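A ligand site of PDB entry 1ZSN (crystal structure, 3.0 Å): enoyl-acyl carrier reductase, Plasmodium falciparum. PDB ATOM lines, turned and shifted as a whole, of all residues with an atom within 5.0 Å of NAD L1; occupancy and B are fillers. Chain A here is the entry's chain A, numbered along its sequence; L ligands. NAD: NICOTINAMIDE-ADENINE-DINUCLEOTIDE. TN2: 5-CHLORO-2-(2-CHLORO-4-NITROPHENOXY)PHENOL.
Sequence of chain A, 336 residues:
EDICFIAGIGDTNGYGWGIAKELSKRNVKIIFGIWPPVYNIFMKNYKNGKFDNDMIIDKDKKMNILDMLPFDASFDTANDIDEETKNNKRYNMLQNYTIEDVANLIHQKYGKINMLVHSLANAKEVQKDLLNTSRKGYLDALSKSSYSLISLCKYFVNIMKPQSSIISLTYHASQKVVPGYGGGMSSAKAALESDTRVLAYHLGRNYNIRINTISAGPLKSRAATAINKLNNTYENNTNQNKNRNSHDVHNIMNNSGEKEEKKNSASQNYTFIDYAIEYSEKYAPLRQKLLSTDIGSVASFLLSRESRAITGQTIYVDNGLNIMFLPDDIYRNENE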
ATOM      1  N   GLY A   8      33.450  -7.354   7.325  1.00  0.00           N
ATOM      2  CA  GLY A   8      32.238  -8.048   6.908  1.00  0.00           C
ATOM      3  C   GLY A   8      32.452  -8.862   5.647  1.00  0.00           C
ATOM      4  O   GLY A   8      32.586  -8.317   4.564  1.00  0.00           O
ATOM      5  N   ILE A   9      32.471 -10.173   5.813  1.00  0.00           N
ATOM      6  CA  ILE A   9      32.743 -11.114   4.739  1.00  0.00           C
ATOM      7  C   ILE A   9      32.706 -12.516   5.366  1.00  0.00           C
ATOM      8  O   ILE A   9      33.369 -12.773   6.378  1.00  0.00           O
ATOM      9  CB  ILE A   9      34.120 -10.832   4.048  1.00  0.00           C
ATOM     10  CG1 ILE A   9      34.406 -11.857   2.960  1.00  0.00           C
ATOM     11  CG2 ILE A   9      35.225 -10.859   5.044  1.00  0.00           C
ATOM     12  CD1 ILE A   9      35.846 -12.327   2.909  1.00  0.00           C
ATOM     13  N   GLY A  10      31.900 -13.418   4.801  1.00  0.00           N
ATOM     14  CA  GLY A  10      31.820 -14.792   5.274  1.00  0.00           C
ATOM     15  C   GLY A  10      32.118 -15.822   4.190  1.00  0.00           C
ATOM     16  O   GLY A  10      32.065 -17.026   4.442  1.00  0.00           O
ATOM     17  N   ASP A  11      32.445 -15.352   2.990  1.00  0.00           N
ATOM     18  CA  ASP A  11      32.661 -16.228   1.840  1.00  0.00           C
ATOM     19  C   ASP A  11      33.225 -15.433   0.687  1.00  0.00           C
ATOM     20  O   ASP A  11      33.560 -14.252   0.840  1.00  0.00           O
ATOM     21  CB  ASP A  11      31.333 -16.856   1.396  1.00  0.00           C
ATOM     22  CG  ASP A  11      30.243 -15.840   1.310  1.00  0.00           C
ATOM     23  OD1 ASP A  11      30.076 -15.148   0.265  1.00  0.00           O
ATOM     24  OD2 ASP A  11      29.553 -15.711   2.325  1.00  0.00           O
ATOM     25  N   GLY A  14      30.468 -12.637  -1.894  1.00  0.00           N
ATOM     26  CA  GLY A  14      30.011 -11.306  -1.507  1.00  0.00           C
ATOM     27  C   GLY A  14      30.762 -10.128  -2.108  1.00  0.00           C
ATOM     28  O   GLY A  14      31.686 -10.308  -2.912  1.00  0.00           O
ATOM     29  N   TYR A  15      30.375  -8.925  -1.696  1.00  0.00           N
ATOM     30  CA  TYR A  15      31.009  -7.686  -2.156  1.00  0.00           C
ATOM     31  C   TYR A  15      32.388  -7.435  -1.584  1.00  0.00           C
ATOM     32  O   TYR A  15      33.301  -7.089  -2.328  1.00  0.00           O
ATOM     33  CB  TYR A  15      30.095  -6.463  -1.967  1.00  0.00           C
ATOM     34  CG  TYR A  15      29.200  -6.190  -3.178  1.00  0.00           C
ATOM     35  CD1 TYR A  15      29.722  -6.162  -4.467  1.00  0.00           C
ATOM     36  CD2 TYR A  15      27.822  -5.968  -3.015  1.00  0.00           C
ATOM     37  CE1 TYR A  15      28.904  -5.944  -5.580  1.00  0.00           C
ATOM     38  CE2 TYR A  15      26.997  -5.743  -4.124  1.00  0.00           C
ATOM     39  CZ  TYR A  15      27.549  -5.726  -5.396  1.00  0.00           C
ATOM     40  OH  TYR A  15      26.761  -5.519  -6.515  1.00  0.00           O
ATOM     41  N   GLY A  16      32.542  -7.599  -0.276  1.00  0.00           N
ATOM     42  CA  GLY A  16      33.859  -7.509   0.361  1.00  0.00           C
ATOM     43  C   GLY A  16      34.947  -8.275  -0.393  1.00  0.00           C
ATOM     44  O   GLY A  16      36.042  -7.760  -0.625  1.00  0.00           O
ATOM     45  N   TRP A  35      32.543 -11.857  11.036  1.00  0.00           N
ATOM     46  CA  TRP A  35      31.537 -12.052  12.077  1.00  0.00           C
ATOM     47  C   TRP A  35      31.900 -13.326  12.818  1.00  0.00           C
ATOM     48  O   TRP A  35      32.061 -14.399  12.207  1.00  0.00           O
ATOM     49  CB  TRP A  35      30.153 -12.163  11.414  1.00  0.00           C
ATOM     50  CG  TRP A  35      28.961 -12.074  12.326  1.00  0.00           C
ATOM     51  CD1 TRP A  35      28.792 -11.215  13.376  1.00  0.00           C
ATOM     52  CD2 TRP A  35      27.749 -12.840  12.248  1.00  0.00           C
ATOM     53  NE1 TRP A  35      27.555 -11.405  13.970  1.00  0.00           N
ATOM     54  CE2 TRP A  35      26.891 -12.394  13.298  1.00  0.00           C
ATOM     55  CE3 TRP A  35      27.312 -13.880  11.399  1.00  0.00           C
ATOM     56  CZ2 TRP A  35      25.610 -12.958  13.522  1.00  0.00           C
ATOM     57  CZ3 TRP A  35      26.029 -14.429  11.623  1.00  0.00           C
ATOM     58  CH2 TRP A  35      25.198 -13.959  12.677  1.00  0.00           C
ATOM     59  N   VAL A  38      30.492 -16.968  11.970  1.00  0.00           N
ATOM     60  CA  VAL A  38      30.958 -17.670  10.776  1.00  0.00           C
ATOM     61  C   VAL A  38      32.473 -17.671  10.661  1.00  0.00           C
ATOM     62  O   VAL A  38      33.007 -18.228   9.710  1.00  0.00           O
ATOM     63  CB  VAL A  38      30.350 -17.106   9.464  1.00  0.00           C
ATOM     64  CG1 VAL A  38      28.841 -17.420   9.386  1.00  0.00           C
ATOM     65  CG2 VAL A  38      30.623 -15.587   9.296  1.00  0.00           C
ATOM     66  N   PHE A  71      35.527 -10.186  14.118  1.00  0.00           N
ATOM     67  CA  PHE A  71      35.162  -8.793  14.215  1.00  0.00           C
ATOM     68  C   PHE A  71      33.658  -8.777  14.296  1.00  0.00           C
ATOM     69  O   PHE A  71      32.971  -9.366  13.451  1.00  0.00           O
ATOM     70  CB  PHE A  71      35.627  -8.053  12.952  1.00  0.00           C
ATOM     71  CG  PHE A  71      35.079  -6.647  12.807  1.00  0.00           C
ATOM     72  CD1 PHE A  71      35.824  -5.554  13.253  1.00  0.00           C
ATOM     73  CD2 PHE A  71      33.836  -6.415  12.228  1.00  0.00           C
ATOM     74  CE1 PHE A  71      35.333  -4.249  13.115  1.00  0.00           C
ATOM     75  CE2 PHE A  71      33.327  -5.098  12.089  1.00  0.00           C
ATOM     76  CZ  PHE A  71      34.092  -4.024  12.524  1.00  0.00           C
ATOM     77  N   ASP A  72      33.144  -8.104  15.321  1.00  0.00           N
ATOM     78  CA  ASP A  72      31.699  -7.967  15.486  1.00  0.00           C
ATOM     79  C   ASP A  72      31.240  -6.519  15.639  1.00  0.00           C
ATOM     80  O   ASP A  72      31.514  -5.871  16.637  1.00  0.00           O
ATOM     81  CB  ASP A  72      31.210  -8.818  16.655  1.00  0.00           C
ATOM     82  CG  ASP A  72      29.708  -8.866  16.717  1.00  0.00           C
ATOM     83  OD1 ASP A  72      29.076  -7.833  16.454  1.00  0.00           O
ATOM     84  OD2 ASP A  72      29.167  -9.948  17.044  1.00  0.00           O
ATOM     85  N   ALA A  73      30.518  -6.047  14.634  1.00  0.00           N
ATOM     86  CA  ALA A  73      30.099  -4.649  14.515  1.00  0.00           C
ATOM     87  C   ALA A  73      29.086  -4.163  15.565  1.00  0.00           C
ATOM     88  O   ALA A  73      28.717  -2.978  15.586  1.00  0.00           O
ATOM     89  CB  ALA A  73      29.535  -4.416  13.107  1.00  0.00           C
ATOM     90  N   SER A  74      28.639  -5.071  16.426  1.00  0.00           N
ATOM     91  CA  SER A  74      27.640  -4.774  17.458  1.00  0.00           C
ATOM     92  C   SER A  74      28.267  -4.151  18.697  1.00  0.00           C
ATOM     93  O   SER A  74      27.605  -3.391  19.416  1.00  0.00           O
ATOM     94  CB  SER A  74      26.912  -6.045  17.886  1.00  0.00           C
ATOM     95  OG  SER A  74      26.571  -6.823  16.751  1.00  0.00           O
ATOM     96  N   SER A 119      31.704  -3.193   4.819  1.00  0.00           N
ATOM     97  CA  SER A 119      30.918  -3.951   3.849  1.00  0.00           C
ATOM     98  C   SER A 119      30.010  -4.951   4.560  1.00  0.00           C
ATOM     99  O   SER A 119      30.061  -6.159   4.280  1.00  0.00           O
ATOM    100  CB  SER A 119      31.820  -4.676   2.853  1.00  0.00           C
ATOM    101  OG  SER A 119      32.544  -5.700   3.509  1.00  0.00           O
ATOM    102  N   LEU A 120      29.188  -4.454   5.475  1.00  0.00           N
ATOM    103  CA  LEU A 120      28.366  -5.323   6.299  1.00  0.00           C
ATOM    104  C   LEU A 120      27.014  -4.740   6.606  1.00  0.00           C
ATOM    105  O   LEU A 120      26.850  -3.526   6.672  1.00  0.00           O
ATOM    106  CB  LEU A 120      29.107  -5.653   7.601  1.00  0.00           C
ATOM    107  CG  LEU A 120      29.368  -4.579   8.668  1.00  0.00           C
ATOM    108  CD1 LEU A 120      28.259  -4.607   9.690  1.00  0.00           C
ATOM    109  CD2 LEU A 120      30.724  -4.819   9.354  1.00  0.00           C
ATOM    110  N   ALA A 121      26.030  -5.622   6.785  1.00  0.00           N
ATOM    111  CA  ALA A 121      24.692  -5.234   7.242  1.00  0.00           C
ATOM    112  C   ALA A 121      24.034  -6.371   8.018  1.00  0.00           C
ATOM    113  O   ALA A 121      24.318  -7.561   7.802  1.00  0.00           O
ATOM    114  CB  ALA A 121      23.821  -4.816   6.064  1.00  0.00           C
ATOM    115  N   ASN A 122      23.153  -5.980   8.932  1.00  0.00           N
ATOM    116  CA  ASN A 122      22.268  -6.907   9.611  1.00  0.00           C
ATOM    117  C   ASN A 122      20.956  -6.234   9.992  1.00  0.00           C
ATOM    118  O   ASN A 122      20.916  -5.094  10.460  1.00  0.00           O
ATOM    119  CB  ASN A 122      22.937  -7.523  10.827  1.00  0.00           C
ATOM    120  CG  ASN A 122      22.600  -8.985  10.996  1.00  0.00           C
ATOM    121  OD1 ASN A 122      23.495  -9.806  11.227  1.00  0.00           O
ATOM    122  ND2 ASN A 122      21.322  -9.332  10.903  1.00  0.00           N
ATOM    123  N   LYS A 144      23.766  -2.300  13.930  1.00  0.00           N
ATOM    124  CA  LYS A 144      24.713  -3.102  13.174  1.00  0.00           C
ATOM    125  C   LYS A 144      25.005  -2.553  11.775  1.00  0.00           C
ATOM    126  O   LYS A 144      26.114  -2.680  11.289  1.00  0.00           O
ATOM    127  CB  LYS A 144      24.274  -4.570  13.146  1.00  0.00           C
ATOM    128  CG  LYS A 144      24.285  -5.174  14.534  1.00  0.00           C
ATOM    129  CD  LYS A 144      23.710  -6.577  14.553  1.00  0.00           C
ATOM    130  CE  LYS A 144      23.454  -7.044  15.981  1.00  0.00           C
ATOM    131  NZ  LYS A 144      22.814  -8.364  15.820  1.00  0.00           N
ATOM    132  N   LEU A 169      29.163   0.508   1.801  1.00  0.00           N
ATOM    133  CA  LEU A 169      28.339   0.050   0.699  1.00  0.00           C
ATOM    134  C   LEU A 169      26.873   0.323   1.021  1.00  0.00           C
ATOM    135  O   LEU A 169      26.382  -0.075   2.070  1.00  0.00           O
ATOM    136  CB  LEU A 169      28.584  -1.428   0.460  1.00  0.00           C
ATOM    137  CG  LEU A 169      29.701  -1.768  -0.526  1.00  0.00           C
ATOM    138  CD1 LEU A 169      31.037  -1.288  -0.052  1.00  0.00           C
ATOM    139  CD2 LEU A 169      29.794  -3.234  -0.740  1.00  0.00           C
ATOM    140  N   THR A 170      26.175   1.019   0.150  1.00  0.00           N
ATOM    141  CA  THR A 170      24.814   1.409   0.454  1.00  0.00           C
ATOM    142  C   THR A 170      23.851   0.817  -0.582  1.00  0.00           C
ATOM    143  O   THR A 170      24.248  -0.050  -1.373  1.00  0.00           O
ATOM    144  CB  THR A 170      24.687   2.955   0.624  1.00  0.00           C
ATOM    145  OG1 THR A 170      23.391   3.291   1.165  1.00  0.00           O
ATOM    146  CG2 THR A 170      24.881   3.695  -0.715  1.00  0.00           C
ATOM    147  N   TYR A 171      22.590   1.255  -0.560  1.00  0.00           N
ATOM    148  CA  TYR A 171      21.601   0.755  -1.505  1.00  0.00           C
ATOM    149  C   TYR A 171      20.378   1.712  -1.727  1.00  0.00           C
ATOM    150  O   TYR A 171      19.843   2.339  -0.793  1.00  0.00           O
ATOM    151  CB  TYR A 171      21.181  -0.669  -1.095  1.00  0.00           C
ATOM    152  CG  TYR A 171      20.182  -1.305  -2.010  1.00  0.00           C
ATOM    153  CD1 TYR A 171      20.475  -1.516  -3.348  1.00  0.00           C
ATOM    154  CD2 TYR A 171      18.919  -1.706  -1.525  1.00  0.00           C
ATOM    155  CE1 TYR A 171      19.544  -2.101  -4.203  1.00  0.00           C
ATOM    156  CE2 TYR A 171      17.983  -2.300  -2.377  1.00  0.00           C
ATOM    157  CZ  TYR A 171      18.308  -2.478  -3.714  1.00  0.00           C
ATOM    158  OH  TYR A 171      17.409  -3.039  -4.580  1.00  0.00           O
ATOM    159  N   TYR A 181      12.559  -4.929   1.028  1.00  0.00           N
ATOM    160  CA  TYR A 181      13.796  -4.521   1.691  1.00  0.00           C
ATOM    161  C   TYR A 181      13.426  -3.836   2.979  1.00  0.00           C
ATOM    162  O   TYR A 181      13.474  -2.606   3.074  1.00  0.00           O
ATOM    163  CB  TYR A 181      14.557  -3.545   0.790  1.00  0.00           C
ATOM    164  CG  TYR A 181      15.990  -3.285   1.147  1.00  0.00           C
ATOM    165  CD1 TYR A 181      16.988  -4.223   0.882  1.00  0.00           C
ATOM    166  CD2 TYR A 181      16.358  -2.079   1.719  1.00  0.00           C
ATOM    167  CE1 TYR A 181      18.326  -3.973   1.195  1.00  0.00           C
ATOM    168  CE2 TYR A 181      17.687  -1.816   2.047  1.00  0.00           C
ATOM    169  CZ  TYR A 181      18.662  -2.756   1.797  1.00  0.00           C
ATOM    170  OH  TYR A 181      19.965  -2.460   2.128  1.00  0.00           O
ATOM    171  N   MET A 185      16.361  -1.848   7.115  1.00  0.00           N
ATOM    172  CA  MET A 185      17.432  -1.738   6.122  1.00  0.00           C
ATOM    173  C   MET A 185      17.425  -0.450   5.295  1.00  0.00           C
ATOM    174  O   MET A 185      18.476   0.146   5.085  1.00  0.00           O
ATOM    175  CB  MET A 185      17.452  -2.945   5.171  1.00  0.00           C
ATOM    176  CG  MET A 185      18.240  -4.128   5.680  1.00  0.00           C
ATOM    177  SD  MET A 185      19.798  -3.677   6.466  1.00  0.00           S
ATOM    178  CE  MET A 185      20.679  -2.888   5.110  1.00  0.00           C
ATOM    179  N   LYS A 189      20.330   2.337   5.575  1.00  0.00           N
ATOM    180  CA  LYS A 189      21.122   2.878   4.463  1.00  0.00           C
ATOM    181  C   LYS A 189      20.890   4.388   4.298  1.00  0.00           C
ATOM    182  O   LYS A 189      21.804   5.131   3.938  1.00  0.00           O
ATOM    183  CB  LYS A 189      20.821   2.116   3.159  1.00  0.00           C
ATOM    184  CG  LYS A 189      21.055   0.620   3.226  1.00  0.00           C
ATOM    185  CD  LYS A 189      22.420   0.251   3.751  1.00  0.00           C
ATOM    186  CE  LYS A 189      22.993  -0.918   2.966  1.00  0.00           C
ATOM    187  NZ  LYS A 189      24.225  -1.499   3.569  1.00  0.00           N
ATOM    188  N   ALA A 216      25.622   0.017  -4.510  1.00  0.00           N
ATOM    189  CA  ALA A 216      25.789  -1.110  -5.394  1.00  0.00           C
ATOM    190  C   ALA A 216      24.455  -1.617  -5.843  1.00  0.00           C
ATOM    191  O   ALA A 216      23.484  -1.522  -5.110  1.00  0.00           O
ATOM    192  CB  ALA A 216      26.510  -2.176  -4.698  1.00  0.00           C
ATOM    193  N   GLY A 217      24.421  -2.137  -7.065  1.00  0.00           N
ATOM    194  CA  GLY A 217      23.236  -2.829  -7.571  1.00  0.00           C
ATOM    195  C   GLY A 217      23.209  -4.238  -7.021  1.00  0.00           C
ATOM    196  O   GLY A 217      23.944  -4.532  -6.087  1.00  0.00           O
ATOM    197  N   PRO A 218      22.390  -5.121  -7.591  1.00  0.00           N
ATOM    198  CA  PRO A 218      22.199  -6.367  -6.867  1.00  0.00           C
ATOM    199  C   PRO A 218      23.279  -7.411  -7.177  1.00  0.00           C
ATOM    200  O   PRO A 218      23.781  -7.519  -8.323  1.00  0.00           O
ATOM    201  CB  PRO A 218      20.845  -6.842  -7.354  1.00  0.00           C
ATOM    202  CG  PRO A 218      20.792  -6.364  -8.787  1.00  0.00           C
ATOM    203  CD  PRO A 218      21.634  -5.105  -8.858  1.00  0.00           C
ATOM    204  N   LEU A 219      23.643  -8.147  -6.136  1.00  0.00           N
ATOM    205  CA  LEU A 219      24.544  -9.278  -6.240  1.00  0.00           C
ATOM    206  C   LEU A 219      24.014 -10.437  -5.413  1.00  0.00           C
ATOM    207  O   LEU A 219      23.569 -10.253  -4.274  1.00  0.00           O
ATOM    208  CB  LEU A 219      25.929  -8.886  -5.743  1.00  0.00           C
ATOM    209  CG  LEU A 219      27.014  -9.929  -6.020  1.00  0.00           C
ATOM    210  CD1 LEU A 219      27.290 -10.016  -7.523  1.00  0.00           C
ATOM    211  CD2 LEU A 219      28.263  -9.568  -5.254  1.00  0.00           C
ATOM    212  N   LYS A 220      24.065 -11.635  -6.003  1.00  0.00           N
ATOM    213  CA  LYS A 220      23.630 -12.857  -5.326  1.00  0.00           C
ATOM    214  C   LYS A 220      24.623 -13.293  -4.249  1.00  0.00           C
ATOM    215  O   LYS A 220      25.305 -14.298  -4.425  1.00  0.00           O
ATOM    216  CB  LYS A 220      23.412 -13.976  -6.345  1.00  0.00           C
ATOM    217  CG  LYS A 220      22.622 -15.144  -5.803  1.00  0.00           C
ATOM    218  CD  LYS A 220      21.764 -15.790  -6.880  1.00  0.00           C
ATOM    219  CE  LYS A 220      20.753 -16.767  -6.259  1.00  0.00           C
ATOM    220  NZ  LYS A 220      20.003 -16.180  -5.076  1.00  0.00           N
ATOM    221  N   SER A 221      24.720 -12.548  -3.145  1.00  0.00           N
ATOM    222  CA  SER A 221      25.542 -12.936  -1.998  1.00  0.00           C
ATOM    223  C   SER A 221      24.707 -13.697  -0.984  1.00  0.00           C
ATOM    224  O   SER A 221      23.483 -13.769  -1.110  1.00  0.00           O
ATOM    225  CB  SER A 221      26.159 -11.703  -1.351  1.00  0.00           C
ATOM    226  OG  SER A 221      25.203 -10.677  -1.191  1.00  0.00           O
ATOM    227  N   ARG A 222      25.352 -14.276   0.043  1.00  0.00           N
ATOM    228  CA  ARG A 222      24.615 -15.076   1.033  1.00  0.00           C
ATOM    229  C   ARG A 222      23.637 -14.206   1.828  1.00  0.00           C
ATOM    230  O   ARG A 222      22.542 -14.649   2.149  1.00  0.00           O
ATOM    231  CB  ARG A 222      25.549 -15.890   1.965  1.00  0.00           C
ATOM    232  CG  ARG A 222      24.831 -16.953   2.881  1.00  0.00           C
ATOM    233  CD  ARG A 222      24.651 -16.494   4.364  1.00  0.00           C
ATOM    234  NE  ARG A 222      23.477 -17.096   5.035  1.00  0.00           N
ATOM    235  CZ  ARG A 222      23.006 -16.743   6.237  1.00  0.00           C
ATOM    236  NH1 ARG A 222      23.591 -15.783   6.950  1.00  0.00           N
ATOM    237  NH2 ARG A 222      21.921 -17.345   6.743  1.00  0.00           N
ATOM    238  N   ALA A 223      24.024 -12.967   2.109  1.00  0.00           N
ATOM    239  CA  ALA A 223      23.161 -12.057   2.826  1.00  0.00           C
ATOM    240  C   ALA A 223      21.908 -11.801   2.025  1.00  0.00           C
ATOM    241  O   ALA A 223      20.804 -11.751   2.574  1.00  0.00           O
ATOM    242  CB  ALA A 223      23.881 -10.777   3.118  1.00  0.00           C
ATOM    243  N   ALA A 224      22.080 -11.640   0.711  1.00  0.00           N
ATOM    244  CA  ALA A 224      20.994 -11.276  -0.194  1.00  0.00           C
ATOM    245  C   ALA A 224      20.017 -12.418  -0.379  1.00  0.00           C
ATOM    246  O   ALA A 224      18.814 -12.175  -0.557  1.00  0.00           O
ATOM    247  CB  ALA A 224      21.562 -10.839  -1.522  1.00  0.00           C
ATOM    248  N   ILE A 273      16.057 -11.126  -4.447  1.00  0.00           N
ATOM    249  CA  ILE A 273      17.343 -10.832  -5.081  1.00  0.00           C
ATOM    250  C   ILE A 273      17.314 -11.375  -6.494  1.00  0.00           C
ATOM    251  O   ILE A 273      17.896 -10.795  -7.403  1.00  0.00           O
ATOM    252  CB  ILE A 273      18.554 -11.442  -4.331  1.00  0.00           C
ATOM    253  CG1 ILE A 273      19.852 -10.781  -4.776  1.00  0.00           C
ATOM    254  CG2 ILE A 273      18.667 -12.940  -4.556  1.00  0.00           C
ATOM    255  CD1 ILE A 273      19.981  -9.312  -4.443  1.00  0.00           C
HETATM  256  PA  NAD L   1      27.565 -10.475   2.506  1.00  0.00           P
HETATM  257  O1A NAD L   1      26.897 -11.637   3.172  1.00  0.00           O
HETATM  258  O2A NAD L   1      28.757 -10.678   1.603  1.00  0.00           O
HETATM  259  O5B NAD L   1      28.043  -9.456   3.652  1.00  0.00           O
HETATM  260  C5B NAD L   1      27.291  -9.232   4.818  1.00  0.00           C
HETATM  261  C4B NAD L   1      28.223  -9.552   5.961  1.00  0.00           C
HETATM  262  O4B NAD L   1      27.800  -8.860   7.117  1.00  0.00           O
HETATM  263  C3B NAD L   1      28.176 -11.007   6.396  1.00  0.00           C
HETATM  264  O3B NAD L   1      29.076 -11.800   5.622  1.00  0.00           O
HETATM  265  C2B NAD L   1      28.611 -10.969   7.853  1.00  0.00           C
HETATM  266  O2B NAD L   1      30.023 -11.234   7.933  1.00  0.00           O
HETATM  267  C1B NAD L   1      28.462  -9.514   8.198  1.00  0.00           C
HETATM  268  N9A NAD L   1      27.805  -9.200   9.487  1.00  0.00           N
HETATM  269  C8A NAD L   1      26.468  -9.229   9.727  1.00  0.00           C
HETATM  270  N7A NAD L   1      26.221  -8.837  11.020  1.00  0.00           N
HETATM  271  C5A NAD L   1      27.410  -8.562  11.616  1.00  0.00           C
HETATM  272  C6A NAD L   1      27.806  -8.125  12.875  1.00  0.00           C
HETATM  273  N6A NAD L   1      26.859  -7.903  13.833  1.00  0.00           N
HETATM  274  N1A NAD L   1      29.148  -7.947  13.107  1.00  0.00           N
HETATM  275  C2A NAD L   1      30.094  -8.162  12.162  1.00  0.00           C
HETATM  276  N3A NAD L   1      29.766  -8.585  10.918  1.00  0.00           N
HETATM  277  C4A NAD L   1      28.460  -8.796  10.594  1.00  0.00           C
HETATM  278  O3  NAD L   1      26.433  -9.689   1.643  1.00  0.00           O
HETATM  279  PN  NAD L   1      26.702  -8.388   0.722  1.00  0.00           P
HETATM  280  O1N NAD L   1      25.395  -8.064   0.057  1.00  0.00           O
HETATM  281  O2N NAD L   1      27.925  -8.573  -0.131  1.00  0.00           O
HETATM  282  O5D NAD L   1      26.992  -7.281   1.863  1.00  0.00           O
HETATM  283  C5D NAD L   1      27.990  -6.277   1.736  1.00  0.00           C
HETATM  284  C4D NAD L   1      27.386  -4.868   1.699  1.00  0.00           C
HETATM  285  O4D NAD L   1      26.899  -4.562   0.379  1.00  0.00           O
HETATM  286  C3D NAD L   1      26.202  -4.756   2.639  1.00  0.00           C
HETATM  287  O3D NAD L   1      26.235  -3.533   3.363  1.00  0.00           O
HETATM  288  C2D NAD L   1      25.012  -4.730   1.709  1.00  0.00           C
HETATM  289  O2D NAD L   1      23.976  -4.038   2.388  1.00  0.00           O
HETATM  290  C1D NAD L   1      25.595  -3.984   0.513  1.00  0.00           C
HETATM  291  N1N NAD L   1      24.833  -4.146  -0.724  1.00  0.00           N
HETATM  292  C2N NAD L   1      24.653  -5.367  -1.283  1.00  0.00           C
HETATM  293  C3N NAD L   1      23.925  -5.539  -2.469  1.00  0.00           C
HETATM  294  C7N NAD L   1      23.686  -6.902  -3.074  1.00  0.00           C
HETATM  295  O7N NAD L   1      22.780  -7.024  -4.019  1.00  0.00           O
HETATM  296  N7N NAD L   1      24.284  -7.943  -2.694  1.00  0.00           N
HETATM  297  C4N NAD L   1      23.390  -4.402  -3.064  1.00  0.00           C
HETATM  298  C5N NAD L   1      23.601  -3.148  -2.480  1.00  0.00           C
HETATM  299  C6N NAD L   1      24.331  -3.047  -1.301  1.00  0.00           C
HETATM  300  O19 TN2 L   2      20.670  -8.235   7.541  1.00  0.00           O
HETATM  301  N17 TN2 L   2      20.066  -8.263   6.489  1.00  0.00           N
HETATM  302  O18 TN2 L   2      18.900  -8.612   6.491  1.00  0.00           O
HETATM  303  C14 TN2 L   2      20.688  -7.883   5.274  1.00  0.00           C
HETATM  304  C13 TN2 L   2      22.086  -7.918   5.143  1.00  0.00           C
HETATM  305  C11 TN2 L   2      22.672  -7.534   3.938  1.00  0.00           C
HETATM  306 CL12 TN2 L   2      24.454  -7.531   3.676  1.00  0.00          CL
HETATM  307  C15 TN2 L   2      19.899  -7.462   4.209  1.00  0.00           C
HETATM  308  C16 TN2 L   2      20.507  -7.076   3.014  1.00  0.00           C
HETATM  309  C10 TN2 L   2      21.895  -7.119   2.878  1.00  0.00           C
HETATM  310  O9  TN2 L   2      22.555  -6.748   1.722  1.00  0.00           O
HETATM  311  C6  TN2 L   2      21.858  -6.446   0.573  1.00  0.00           C
HETATM  312  C4  TN2 L   2      21.471  -5.133   0.309  1.00  0.00           C
HETATM  313  O5  TN2 L   2      21.758  -4.102   1.149  1.00  0.00           O
HETATM  314  C3  TN2 L   2      20.769  -4.839  -0.860  1.00  0.00           C
HETATM  315  C7  TN2 L   2      21.539  -7.481  -0.317  1.00  0.00           C
HETATM  316  C8  TN2 L   2      20.825  -7.189  -1.479  1.00  0.00           C
HETATM  317  C2  TN2 L   2      20.448  -5.867  -1.738  1.00  0.00           C
HETATM  318 CL20 TN2 L   2      19.554  -5.441  -3.211  1.00  0.00          CL
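O of Thr 170 sits at hydrogen-bond distance from N of Ala 216.
OD1 of Asp 11 lies within hydrogen-bond range of N of Gly 14, 3.3 Å away.
The side-chain hydroxyl (OG) of Ser 74 sits at hydrogen-bond distance from the side-chain carboxylate (OD1) of Asp 72.
The backbone carbonyl oxygen (O) of Gly 8 sits at hydrogen-bond distance from the side-chain hydroxyl (OG) of Ser 119 (2.8 Å).
O of Leu 169 sits at hydrogen-bond distance from NZ of Lys 189 (3.0 Å).
The backbone NH (N) of Trp 35 lies close to the backbone carbonyl oxygen (O) of Phe 71 (3.5 Å).
The side-chain hydroxyl (OH) of Tyr 15 sits at hydrogen-bond distance from the backbone carbonyl oxygen (O) of Gly 217, 3.0 Å away.
O of Gly 217 lies close to O7N of NAD L1 (3.4 Å).
Residues that only touch NAD L1: Gly 14 (3.4 Å), Trp 35 (3.3 Å), Phe 71 (3.4 Å), Ser 119 (3.3 Å), Ala 121 (3.3 Å), Lys 144 (3.5 Å), Leu 169 (3.4 Å), Thr 170 (3.0 Å), Tyr 171 (3.6 Å), Ala 216 (3.1 Å), Pro 218 (3.0 Å) and Ile 273 (3.6 Å).
Within 4 Å of NAD L1: Ile 9, Gly 10, Gly 14, Tyr 15, Trp 35, Phe 71, Asp 72, Ala 73, Ser 74, Ser 119, Leu 120, Ala 121, Asn 122, Lys 144, Leu 169, Thr 170, Tyr 171, Lys 189, Ala 216, Gly 217, Pro 218, Leu 219, Ser 221, Ala 223 and Ile 273.
Along chain A the residues within 4 Å of NAD L1 span positions 9 to 273.
O5 of TN2 L2 lies within hydrogen-bond range of O2D of NAD L1.
The side-chain hydroxyl (OG) of Ser 221 sits at hydrogen-bond distance from an oxygen (O1N) of NAD L1 (2.9 Å).
An oxygen (O3B) of NAD L1 sits at hydrogen-bond distance from the backbone NH of Gly 10 (3.4 Å).
The backbone NH (N) of Leu 219 sits at hydrogen-bond distance from an oxygen (O7N) of NAD L1 (2.5 Å).
An oxygen (O3D) of NAD L1 sits at hydrogen-bond distance from the backbone carbonyl oxygen (O) of Leu 120 (3.4 Å).
N6A of NAD L1 is in hydrogen-bond range of OD1 of Asp 72 (3.4 Å).
A nitrogen (N7N) of NAD L1 sits at hydrogen-bond distance from the backbone carbonyl oxygen (O) of Leu 219.
An oxygen (O5) of TN2 L2 is in hydrogen-bond range of the side-chain hydroxyl (OH) of Tyr 181 (2.6 Å).
O2B of NAD L1 lies within hydrogen-bond range of N of Ile 9 (3.4 Å).
An oxygen (O1A) of NAD L1 sits close to the backbone NH of Ala 223 (3.3 Å).
The backbone NH of Tyr 15 lies within hydrogen-bond range of an oxygen (O2N) of NAD L1, at 2.9 Å.
The side-chain amino group (NZ) of Lys 189 sits at hydrogen-bond distance from an oxygen (O2D) of NAD L1, 2.8 Å away.
The side-chain amide oxygen of Asn 122 lies close to a nitrogen (N7A) of NAD L1.
The side-chain hydroxyl (OG) of Ser 74 lies within hydrogen-bond range of a nitrogen (N6A) of NAD L1.
A nitrogen (N1A) of NAD L1 is in hydrogen-bond range of the backbone NH (N) of Ala 73.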
